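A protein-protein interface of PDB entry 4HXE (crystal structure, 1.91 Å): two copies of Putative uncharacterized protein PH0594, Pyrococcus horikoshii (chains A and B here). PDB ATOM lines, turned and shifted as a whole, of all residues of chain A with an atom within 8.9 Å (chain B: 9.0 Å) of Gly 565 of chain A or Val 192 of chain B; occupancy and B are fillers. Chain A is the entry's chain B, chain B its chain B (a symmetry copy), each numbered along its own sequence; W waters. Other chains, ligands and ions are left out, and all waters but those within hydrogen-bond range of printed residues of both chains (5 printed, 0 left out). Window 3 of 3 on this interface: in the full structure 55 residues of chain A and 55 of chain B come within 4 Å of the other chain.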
ATOM      1  N   ALA A 531       6.127  13.136  -2.867  1.00  0.00           N
ATOM      2  CA  ALA A 531       6.319  13.785  -4.162  1.00  0.00           C
ATOM      3  C   ALA A 531       7.236  14.994  -4.079  1.00  0.00           C
ATOM      4  O   ALA A 531       7.989  15.194  -5.014  1.00  0.00           O
ATOM      5  CB  ALA A 531       4.973  14.160  -4.792  1.00  0.00           C
ATOM      6  N   LYS A 532       7.163  15.814  -2.998  1.00  0.00           N
ATOM      7  CA  LYS A 532       8.064  16.967  -2.852  1.00  0.00           C
ATOM      8  C   LYS A 532       9.561  16.608  -3.019  1.00  0.00           C
ATOM      9  O   LYS A 532      10.352  17.419  -3.406  1.00  0.00           O
ATOM     10  CB  LYS A 532       7.870  17.617  -1.483  1.00  0.00           C
ATOM     11  CG  LYS A 532       6.558  18.376  -1.327  1.00  0.00           C
ATOM     12  CD  LYS A 532       6.460  19.003   0.056  1.00  0.00           C
ATOM     13  CE  LYS A 532       5.410  20.095   0.052  1.00  0.00           C
ATOM     14  NZ  LYS A 532       5.013  20.378   1.452  1.00  0.00           N
ATOM     15  N   VAL A 534      10.994  14.613  -5.034  1.00  0.00           N
ATOM     16  CA  VAL A 534      11.436  14.237  -6.383  1.00  0.00           C
ATOM     17  C   VAL A 534      12.335  15.309  -7.038  1.00  0.00           C
ATOM     18  O   VAL A 534      12.017  16.538  -7.008  1.00  0.00           O
ATOM     19  CB  VAL A 534      10.229  13.845  -7.284  1.00  0.00           C
ATOM     20  CG1 VAL A 534      10.686  13.676  -8.757  1.00  0.00           C
ATOM     21  CG2 VAL A 534       9.559  12.583  -6.734  1.00  0.00           C
ATOM     22  N   LYS A 535      13.456  14.873  -7.608  1.00  0.00           N
ATOM     23  CA  LYS A 535      14.317  15.823  -8.281  1.00  0.00           C
ATOM     24  C   LYS A 535      14.632  15.391  -9.707  1.00  0.00           C
ATOM     25  O   LYS A 535      15.195  16.180 -10.397  1.00  0.00           O
ATOM     26  CB  LYS A 535      15.651  16.032  -7.549  1.00  0.00           C
ATOM     27  CG  LYS A 535      15.556  16.626  -6.152  1.00  0.00           C
ATOM     28  CD  LYS A 535      16.939  16.654  -5.420  1.00  0.00           C
ATOM     29  N   TYR A 558       1.235  12.331 -11.353  1.00  0.00           N
ATOM     30  CA  TYR A 558       1.595  13.273 -12.371  1.00  0.00           C
ATOM     31  C   TYR A 558       1.086  14.667 -11.955  1.00  0.00           C
ATOM     32  O   TYR A 558       1.857  15.616 -11.926  1.00  0.00           O
ATOM     33  CB  TYR A 558       0.953  12.889 -13.731  1.00  0.00           C
ATOM     34  CG  TYR A 558       1.094  14.018 -14.725  1.00  0.00           C
ATOM     35  CD1 TYR A 558       2.345  14.252 -15.336  1.00  0.00           C
ATOM     36  CD2 TYR A 558       0.047  14.855 -15.006  1.00  0.00           C
ATOM     37  CE1 TYR A 558       2.532  15.288 -16.218  1.00  0.00           C
ATOM     38  CE2 TYR A 558       0.210  15.899 -15.898  1.00  0.00           C
ATOM     39  CZ  TYR A 558       1.457  16.105 -16.503  1.00  0.00           C
ATOM     40  OH  TYR A 558       1.689  17.186 -17.345  1.00  0.00           O
ATOM     41  N   HIS A 559      -0.211  14.773 -11.603  1.00  0.00           N
ATOM     42  CA  HIS A 559      -0.793  16.048 -11.237  1.00  0.00           C
ATOM     43  C   HIS A 559      -0.104  16.632  -9.993  1.00  0.00           C
ATOM     44  O   HIS A 559       0.173  17.840  -9.928  1.00  0.00           O
ATOM     45  CB  HIS A 559      -2.286  15.880 -10.881  1.00  0.00           C
ATOM     46  CG  HIS A 559      -3.162  15.795 -12.049  1.00  0.00           C
ATOM     47  ND1 HIS A 559      -4.388  15.199 -11.999  1.00  0.00           N
ATOM     48  CD2 HIS A 559      -3.007  16.300 -13.364  1.00  0.00           C
ATOM     49  CE1 HIS A 559      -4.988  15.300 -13.233  1.00  0.00           C
ATOM     50  NE2 HIS A 559      -4.137  15.958 -14.072  1.00  0.00           N
ATOM     51  N   VAL A 560       0.119  15.816  -8.972  1.00  0.00           N
ATOM     52  CA  VAL A 560       0.727  16.349  -7.718  1.00  0.00           C
ATOM     53  C   VAL A 560       2.191  16.787  -7.992  1.00  0.00           C
ATOM     54  O   VAL A 560       2.623  17.869  -7.571  1.00  0.00           O
ATOM     55  CB  VAL A 560       0.636  15.315  -6.577  1.00  0.00           C
ATOM     56  CG1 VAL A 560       1.528  15.657  -5.405  1.00  0.00           C
ATOM     57  CG2 VAL A 560      -0.834  15.170  -6.134  1.00  0.00           C
ATOM     58  N   LEU A 561       2.927  15.960  -8.725  1.00  0.00           N
ATOM     59  CA  LEU A 561       4.284  16.352  -9.152  1.00  0.00           C
ATOM     60  C   LEU A 561       4.221  17.645  -9.919  1.00  0.00           C
ATOM     61  O   LEU A 561       5.096  18.476  -9.681  1.00  0.00           O
ATOM     62  CB  LEU A 561       4.979  15.279 -10.009  1.00  0.00           C
ATOM     63  CG  LEU A 561       5.409  13.995  -9.276  1.00  0.00           C
ATOM     64  CD1 LEU A 561       5.870  12.931 -10.260  1.00  0.00           C
ATOM     65  CD2 LEU A 561       6.561  14.341  -8.336  1.00  0.00           C
ATOM     66  N   LYS A 562       3.237  17.848 -10.836  1.00  0.00           N
ATOM     67  CA  LYS A 562       3.148  19.183 -11.544  1.00  0.00           C
ATOM     68  C   LYS A 562       2.813  20.290 -10.554  1.00  0.00           C
ATOM     69  O   LYS A 562       3.322  21.407 -10.634  1.00  0.00           O
ATOM     70  CB  LYS A 562       2.112  19.219 -12.684  1.00  0.00           C
ATOM     71  CG  LYS A 562       2.443  18.283 -13.846  1.00  0.00           C
ATOM     72  CD  LYS A 562       3.677  18.740 -14.640  1.00  0.00           C
ATOM     73  CE  LYS A 562       3.499  20.120 -15.207  1.00  0.00           C
ATOM     74  NZ  LYS A 562       4.658  20.440 -16.124  1.00  0.00           N
ATOM     75  N   ASP A 563       1.967  19.962  -9.580  1.00  0.00           N
ATOM     76  CA  ASP A 563       1.527  20.974  -8.621  1.00  0.00           C
ATOM     77  C   ASP A 563       2.757  21.417  -7.793  1.00  0.00           C
ATOM     78  O   ASP A 563       2.712  22.460  -7.176  1.00  0.00           O
ATOM     79  CB  ASP A 563       0.422  20.398  -7.704  1.00  0.00           C
ATOM     80  CG  ASP A 563      -0.474  21.479  -7.062  1.00  0.00           C
ATOM     81  OD1 ASP A 563      -0.680  22.582  -7.593  1.00  0.00           O
ATOM     82  OD2 ASP A 563      -1.062  21.199  -5.994  1.00  0.00           O
ATOM     83  N   LEU A 564       3.803  20.573  -7.731  1.00  0.00           N
ATOM     84  CA  LEU A 564       4.987  20.870  -6.939  1.00  0.00           C
ATOM     85  C   LEU A 564       6.089  21.386  -7.865  1.00  0.00           C
ATOM     86  O   LEU A 564       7.199  21.517  -7.431  1.00  0.00           O
ATOM     87  CB  LEU A 564       5.433  19.644  -6.118  1.00  0.00           C
ATOM     88  CG  LEU A 564       4.408  19.180  -5.052  1.00  0.00           C
ATOM     89  CD1 LEU A 564       4.656  17.768  -4.474  1.00  0.00           C
ATOM     90  CD2 LEU A 564       4.302  20.247  -3.933  1.00  0.00           C
ATOM     91  N   GLY A 565       5.806  21.671  -9.147  1.00  0.00           N
ATOM     92  CA  GLY A 565       6.859  22.282  -9.989  1.00  0.00           C
ATOM     93  C   GLY A 565       7.843  21.291 -10.549  1.00  0.00           C
ATOM     94  O   GLY A 565       8.881  21.691 -11.090  1.00  0.00           O
ATOM     95  N   LYS A 566       7.550  20.003 -10.462  1.00  0.00           N
ATOM     96  CA  LYS A 566       8.490  18.991 -10.919  1.00  0.00           C
ATOM     97  C   LYS A 566       8.411  18.770 -12.441  1.00  0.00           C
ATOM     98  O   LYS A 566       7.349  19.010 -13.055  1.00  0.00           O
ATOM     99  CB  LYS A 566       8.243  17.621 -10.205  1.00  0.00           C
ATOM    100  CG  LYS A 566       8.079  17.684  -8.702  1.00  0.00           C
ATOM    101  CD  LYS A 566       9.216  18.432  -8.002  1.00  0.00           C
ATOM    102  CE  LYS A 566       9.115  18.244  -6.496  1.00  0.00           C
ATOM    103  NZ  LYS A 566      10.462  18.557  -5.948  1.00  0.00           N
ATOM    104  N   GLU A 567       9.539  18.351 -13.035  1.00  0.00           N
ATOM    105  CA  GLU A 567       9.565  17.996 -14.457  1.00  0.00           C
ATOM    106  C   GLU A 567       9.034  16.556 -14.608  1.00  0.00           C
ATOM    107  O   GLU A 567       9.691  15.580 -14.179  1.00  0.00           O
ATOM    108  CB  GLU A 567      10.983  18.088 -15.040  1.00  0.00           C
ATOM    109  CG  GLU A 567      10.966  17.668 -16.499  1.00  0.00           C
ATOM    110  CD  GLU A 567      12.298  17.756 -17.197  1.00  0.00           C
ATOM    111  OE1 GLU A 567      12.296  17.373 -18.369  1.00  0.00           O
ATOM    112  OE2 GLU A 567      13.321  18.200 -16.627  1.00  0.00           O
ATOM    113  N   VAL A 568       7.827  16.439 -15.149  1.00  0.00           N
ATOM    114  CA  VAL A 568       7.199  15.126 -15.237  1.00  0.00           C
ATOM    115  C   VAL A 568       6.304  15.146 -16.461  1.00  0.00           C
ATOM    116  O   VAL A 568       5.779  16.217 -16.859  1.00  0.00           O
ATOM    117  CB  VAL A 568       6.377  14.774 -13.956  1.00  0.00           C
ATOM    118  CG1 VAL A 568       5.288  15.811 -13.748  1.00  0.00           C
ATOM    119  CG2 VAL A 568       5.773  13.311 -14.035  1.00  0.00           C
ATOM    120  N   ASP B 135       2.037  17.363 -20.653  1.00  0.00           N
ATOM    121  CA  ASP B 135       3.163  17.980 -19.944  1.00  0.00           C
ATOM    122  C   ASP B 135       2.714  19.197 -19.159  1.00  0.00           C
ATOM    123  O   ASP B 135       3.541  19.887 -18.543  1.00  0.00           O
ATOM    124  CB  ASP B 135       4.237  18.423 -20.923  1.00  0.00           C
ATOM    125  CG  ASP B 135       3.658  19.174 -22.130  1.00  0.00           C
ATOM    126  OD1 ASP B 135       4.489  19.528 -22.944  1.00  0.00           O
ATOM    127  OD2 ASP B 135       2.414  19.273 -22.360  1.00  0.00           O
ATOM    128  N   ASP B 136       1.413  19.450 -19.195  1.00  0.00           N
ATOM    129  CA  ASP B 136       0.826  20.560 -18.415  1.00  0.00           C
ATOM    130  C   ASP B 136      -0.218  19.980 -17.456  1.00  0.00           C
ATOM    131  O   ASP B 136      -0.158  18.794 -17.101  1.00  0.00           O
ATOM    132  CB  ASP B 136       0.234  21.622 -19.384  1.00  0.00           C
ATOM    133  CG  ASP B 136       0.132  23.067 -18.774  1.00  0.00           C
ATOM    134  OD1 ASP B 136       0.235  23.306 -17.578  1.00  0.00           O
ATOM    135  OD2 ASP B 136      -0.152  23.997 -19.508  1.00  0.00           O
ATOM    136  N   VAL B 137      -1.106  20.808 -16.942  1.00  0.00           N
ATOM    137  CA  VAL B 137      -2.134  20.289 -16.028  1.00  0.00           C
ATOM    138  C   VAL B 137      -3.388  21.081 -16.286  1.00  0.00           C
ATOM    139  O   VAL B 137      -3.285  22.224 -16.702  1.00  0.00           O
ATOM    140  CB  VAL B 137      -1.872  20.475 -14.510  1.00  0.00           C
ATOM    141  CG1 VAL B 137      -0.817  19.534 -13.971  1.00  0.00           C
ATOM    142  CG2 VAL B 137      -1.565  21.906 -14.184  1.00  0.00           C
ATOM    143  N   HIS B 189      -3.471  32.823 -15.888  1.00  0.00           N
ATOM    144  CA  HIS B 189      -2.148  33.241 -15.495  1.00  0.00           C
ATOM    145  C   HIS B 189      -1.326  32.019 -15.060  1.00  0.00           C
ATOM    146  O   HIS B 189      -1.801  31.143 -14.324  1.00  0.00           O
ATOM    147  CB  HIS B 189      -2.271  34.284 -14.393  1.00  0.00           C
ATOM    148  CG  HIS B 189      -0.964  34.736 -13.888  1.00  0.00           C
ATOM    149  ND1 HIS B 189      -0.251  35.737 -14.478  1.00  0.00           N
ATOM    150  CD2 HIS B 189      -0.155  34.206 -12.885  1.00  0.00           C
ATOM    151  CE1 HIS B 189       0.929  35.860 -13.840  1.00  0.00           C
ATOM    152  NE2 HIS B 189       0.980  34.942 -12.868  1.00  0.00           N
ATOM    153  N   ARG B 190      -0.078  31.937 -15.499  1.00  0.00           N
ATOM    154  CA  ARG B 190       0.730  30.777 -15.154  1.00  0.00           C
ATOM    155  C   ARG B 190       1.663  31.113 -14.012  1.00  0.00           C
ATOM    156  O   ARG B 190       2.479  31.971 -14.139  1.00  0.00           O
ATOM    157  CB  ARG B 190       1.535  30.213 -16.352  1.00  0.00           C
ATOM    158  CG  ARG B 190       2.373  28.964 -15.974  1.00  0.00           C
ATOM    159  CD  ARG B 190       3.042  28.233 -17.158  1.00  0.00           C
ATOM    160  NE  ARG B 190       2.110  27.947 -18.238  1.00  0.00           N
ATOM    161  CZ  ARG B 190       1.449  26.804 -18.409  1.00  0.00           C
ATOM    162  NH1 ARG B 190       1.577  25.798 -17.577  1.00  0.00           N
ATOM    163  NH2 ARG B 190       0.628  26.676 -19.409  1.00  0.00           N
ATOM    164  N   ASP B 191       1.506  30.409 -12.886  1.00  0.00           N
ATOM    165  CA  ASP B 191       2.567  30.348 -11.835  1.00  0.00           C
ATOM    166  C   ASP B 191       3.269  28.973 -11.849  1.00  0.00           C
ATOM    167  O   ASP B 191       3.832  28.602 -12.883  1.00  0.00           O
ATOM    168  CB  ASP B 191       2.052  30.687 -10.444  1.00  0.00           C
ATOM    169  CG  ASP B 191       1.603  32.172 -10.352  1.00  0.00           C
ATOM    170  OD1 ASP B 191       2.281  33.128 -10.844  1.00  0.00           O
ATOM    171  OD2 ASP B 191       0.534  32.341  -9.777  1.00  0.00           O
ATOM    172  N   VAL B 192       3.229  28.210 -10.751  1.00  0.00           N
ATOM    173  CA  VAL B 192       3.745  26.806 -10.837  1.00  0.00           C
ATOM    174  C   VAL B 192       2.864  25.994 -11.817  1.00  0.00           C
ATOM    175  O   VAL B 192       3.350  25.257 -12.630  1.00  0.00           O
ATOM    176  CB  VAL B 192       3.903  26.158  -9.458  1.00  0.00           C
ATOM    177  CG1 VAL B 192       4.417  24.738  -9.633  1.00  0.00           C
ATOM    178  CG2 VAL B 192       4.925  27.011  -8.681  1.00  0.00           C
ATOM    179  N   ILE B 193       1.552  26.236 -11.758  1.00  0.00           N
ATOM    180  CA  ILE B 193       0.571  25.727 -12.722  1.00  0.00           C
ATOM    181  C   ILE B 193      -0.307  26.910 -13.194  1.00  0.00           C
ATOM    182  O   ILE B 193      -0.213  28.004 -12.605  1.00  0.00           O
ATOM    183  CB  ILE B 193      -0.295  24.611 -12.051  1.00  0.00           C
ATOM    184  CG1 ILE B 193      -1.158  25.127 -10.900  1.00  0.00           C
ATOM    185  CG2 ILE B 193       0.585  23.445 -11.575  1.00  0.00           C
ATOM    186  CD1 ILE B 193      -2.187  24.104 -10.380  1.00  0.00           C
ATOM    187  N   PRO B 194      -1.164  26.724 -14.249  1.00  0.00           N
ATOM    188  CA  PRO B 194      -2.106  27.785 -14.616  1.00  0.00           C
ATOM    189  C   PRO B 194      -3.091  28.023 -13.484  1.00  0.00           C
ATOM    190  O   PRO B 194      -3.572  27.059 -12.833  1.00  0.00           O
ATOM    191  CB  PRO B 194      -2.860  27.197 -15.852  1.00  0.00           C
ATOM    192  CG  PRO B 194      -1.867  26.215 -16.427  1.00  0.00           C
ATOM    193  CD  PRO B 194      -1.262  25.586 -15.180  1.00  0.00           C
ATOM    194  N   ARG B 195      -3.406  29.284 -13.254  1.00  0.00           N
ATOM    195  CA  ARG B 195      -4.252  29.604 -12.099  1.00  0.00           C
ATOM    196  C   ARG B 195      -5.751  29.589 -12.540  1.00  0.00           C
ATOM    197  O   ARG B 195      -6.459  30.579 -12.456  1.00  0.00           O
ATOM    198  CB  ARG B 195      -3.772  30.888 -11.404  1.00  0.00           C
ATOM    199  CG  ARG B 195      -2.279  30.842 -11.017  1.00  0.00           C
ATOM    200  CD  ARG B 195      -2.004  29.720  -9.974  1.00  0.00           C
ATOM    201  NE  ARG B 195      -2.792  29.881  -8.735  1.00  0.00           N
ATOM    202  CZ  ARG B 195      -2.546  30.789  -7.756  1.00  0.00           C
ATOM    203  NH1 ARG B 195      -1.589  31.713  -7.883  1.00  0.00           N
ATOM    204  NH2 ARG B 195      -3.303  30.817  -6.659  1.00  0.00           N
ATOM    205  N   LYS B 216      -2.345  39.039 -14.042  1.00  0.00           N
ATOM    206  CA  LYS B 216      -2.737  38.306 -12.849  1.00  0.00           C
ATOM    207  C   LYS B 216      -3.958  38.948 -12.128  1.00  0.00           C
ATOM    208  O   LYS B 216      -3.922  39.306 -10.922  1.00  0.00           O
ATOM    209  CB  LYS B 216      -1.536  38.106 -11.931  1.00  0.00           C
ATOM    210  CG  LYS B 216      -1.795  37.194 -10.744  1.00  0.00           C
ATOM    211  CD  LYS B 216      -0.483  36.851 -10.059  1.00  0.00           C
ATOM    212  CE  LYS B 216      -0.470  35.431  -9.472  1.00  0.00           C
ATOM    213  NZ  LYS B 216       0.972  35.010  -9.443  1.00  0.00           N
ATOM    214  N   LEU B 505      -6.719  20.305  -8.109  1.00  0.00           N
ATOM    215  CA  LEU B 505      -5.439  20.900  -7.729  1.00  0.00           C
ATOM    216  C   LEU B 505      -5.634  22.283  -7.057  1.00  0.00           C
ATOM    217  O   LEU B 505      -4.941  22.610  -6.107  1.00  0.00           O
ATOM    218  CB  LEU B 505      -4.482  20.998  -8.942  1.00  0.00           C
ATOM    219  CG  LEU B 505      -3.752  19.726  -9.439  1.00  0.00           C
ATOM    220  CD1 LEU B 505      -2.673  20.188 -10.402  1.00  0.00           C
ATOM    221  CD2 LEU B 505      -3.138  18.853  -8.292  1.00  0.00           C
ATOM    222  N   LYS B 509      -7.830  22.574  -2.587  1.00  0.00           N
ATOM    223  CA  LYS B 509      -7.023  23.359  -1.662  1.00  0.00           C
ATOM    224  C   LYS B 509      -7.876  24.405  -0.999  1.00  0.00           C
ATOM    225  O   LYS B 509      -7.680  24.686   0.205  1.00  0.00           O
ATOM    226  CB  LYS B 509      -5.839  24.057  -2.353  1.00  0.00           C
ATOM    227  CG  LYS B 509      -4.731  23.040  -2.717  1.00  0.00           C
ATOM    228  CD  LYS B 509      -3.494  23.785  -3.241  1.00  0.00           C
ATOM    229  CE  LYS B 509      -2.357  22.759  -3.484  1.00  0.00           C
ATOM    230  NZ  LYS B 509      -1.209  23.398  -4.215  1.00  0.00           N
HETATM  231  O   HOH W   1      -2.443  23.965  -6.630  1.00  0.00           O
HETATM  232  O   HOH W   2       6.547  18.819 -17.217  1.00  0.00           O
HETATM  233  O   HOH W   3       4.297  22.715 -12.735  1.00  0.00           O
HETATM  234  O   HOH W   4       1.274  22.110  -4.285  1.00  0.00           O
HETATM  235  O   HOH W   5       3.689  22.936 -17.098  1.00  0.00           O
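The side-chain hydroxyl of Tyr 558 of chain A lies close to the backbone NH of Asp 135 of chain B, 3.3 Å away. OH of Tyr 558 of chain A lies within hydrogen-bond range of O of Asp 136 of chain B (2.5 Å). The side-chain amino group (NZ) of Lys 562 of chain A is in hydrogen-bond range of the backbone carbonyl oxygen (O) of Asp 135 of chain B (2.7 Å). NZ of Lys 509 of chain B lies within salt-bridge range of OD2 of Asp 563 of chain A (2.8 Å).
OD2 of Asp 136 of chain B is in salt-bridge range of NH2 of Arg 190 of chain B, 2.8 Å away.
Among the printed residues, merely in contact across the chains: His 559 of chain A with Val 137 of chain B (3.95 Å), His 559 of chain A with Leu 505 of chain B (3.7 Å), Lys 562 of chain A with Val 137 of chain B (3.2 Å), Lys 562 of chain A with Val 192 of chain B (3.6 Å), Lys 562 of chain A with Ile 193 of chain B (3.5 Å), Asp 563 of chain A with Val 192 of chain B (3.8 Å), Asp 563 of chain A with Ile 193 of chain B (3.5 Å), Asp 563 of chain A with Leu 505 of chain B (3.9 Å) and Gly 565 of chain A with Val 192 of chain B (3.4 Å).
Val 560 of chain A touches none of the printed residues of chain B. Of chain B, only Val 192 (3.4 Å) comes within 4 Å of Gly 565 of chain A. Val 192 of chain B touches just these residues of chain A: Lys 562, Asp 563 and Gly 565. Printed residues of chain A within 4 Å of Leu 505 of chain B: His 559 and Asp 563. Of the printed residues of chain A, Lys 509 of chain B touches Asp 563. The nearest residue of chain A that does not touch Val 192 of chain B is Leu 564 of chain A (4.1 Å). The nearest printed residue of chain A that does not touch Asp 135 of chain B is Val 568 of chain A (4.4 Å).
Of the 13 printed residues of chain B, 7 touch a printed residue of chain A. Hydrophobic or aromatic side chains of chain B that line the printed part of chain A: Val 137, Val 192, Ile 193 and Leu 505. Hydrophobic or aromatic side chains of chain A within 4 Å of the printed part of chain B: Tyr 558 and His 559. Along chain A the printed residues that touch a printed residue of chain B span positions 558 to 565. Among the printed residues, Asp or Glu carboxylates within 4 Å of a Lys or Arg side-chain nitrogen of the other chain: Asp 563 of chain A with Lys 509 of chain B.
No position is printed for both chains.
Water W1 lies within hydrogen-bond range of OD1 of Asp 563 of chain A (2.4 Å), NZ of Lys 509 of chain B (2.8 Å) and O of Leu 505 of chain B (2.9 Å). Water W3 bridges O of Lys 562 of chain A (2.7 Å) and O of Val 192 of chain B (2.7 Å). Water W2 lies within hydrogen-bond range of the side-chain amino group (NZ) of Lys 562 of chain A (2.7 Å), the backbone carbonyl oxygen (O) of Val 568 of chain A (2.7 Å) and the backbone carbonyl oxygen (O) of Asp 135 of chain B (3.5 Å). Water W4 lies within hydrogen-bond range of NZ of Lys 509 of chain B (2.8 Å) and OD2 of Asp 563 of chain A (3.0 Å). Water W5 lies within hydrogen-bond range of the side-chain amino group of Lys 562 of chain A (2.8 Å) and the backbone carbonyl oxygen of Asp 135 of chain B (3.4 Å).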
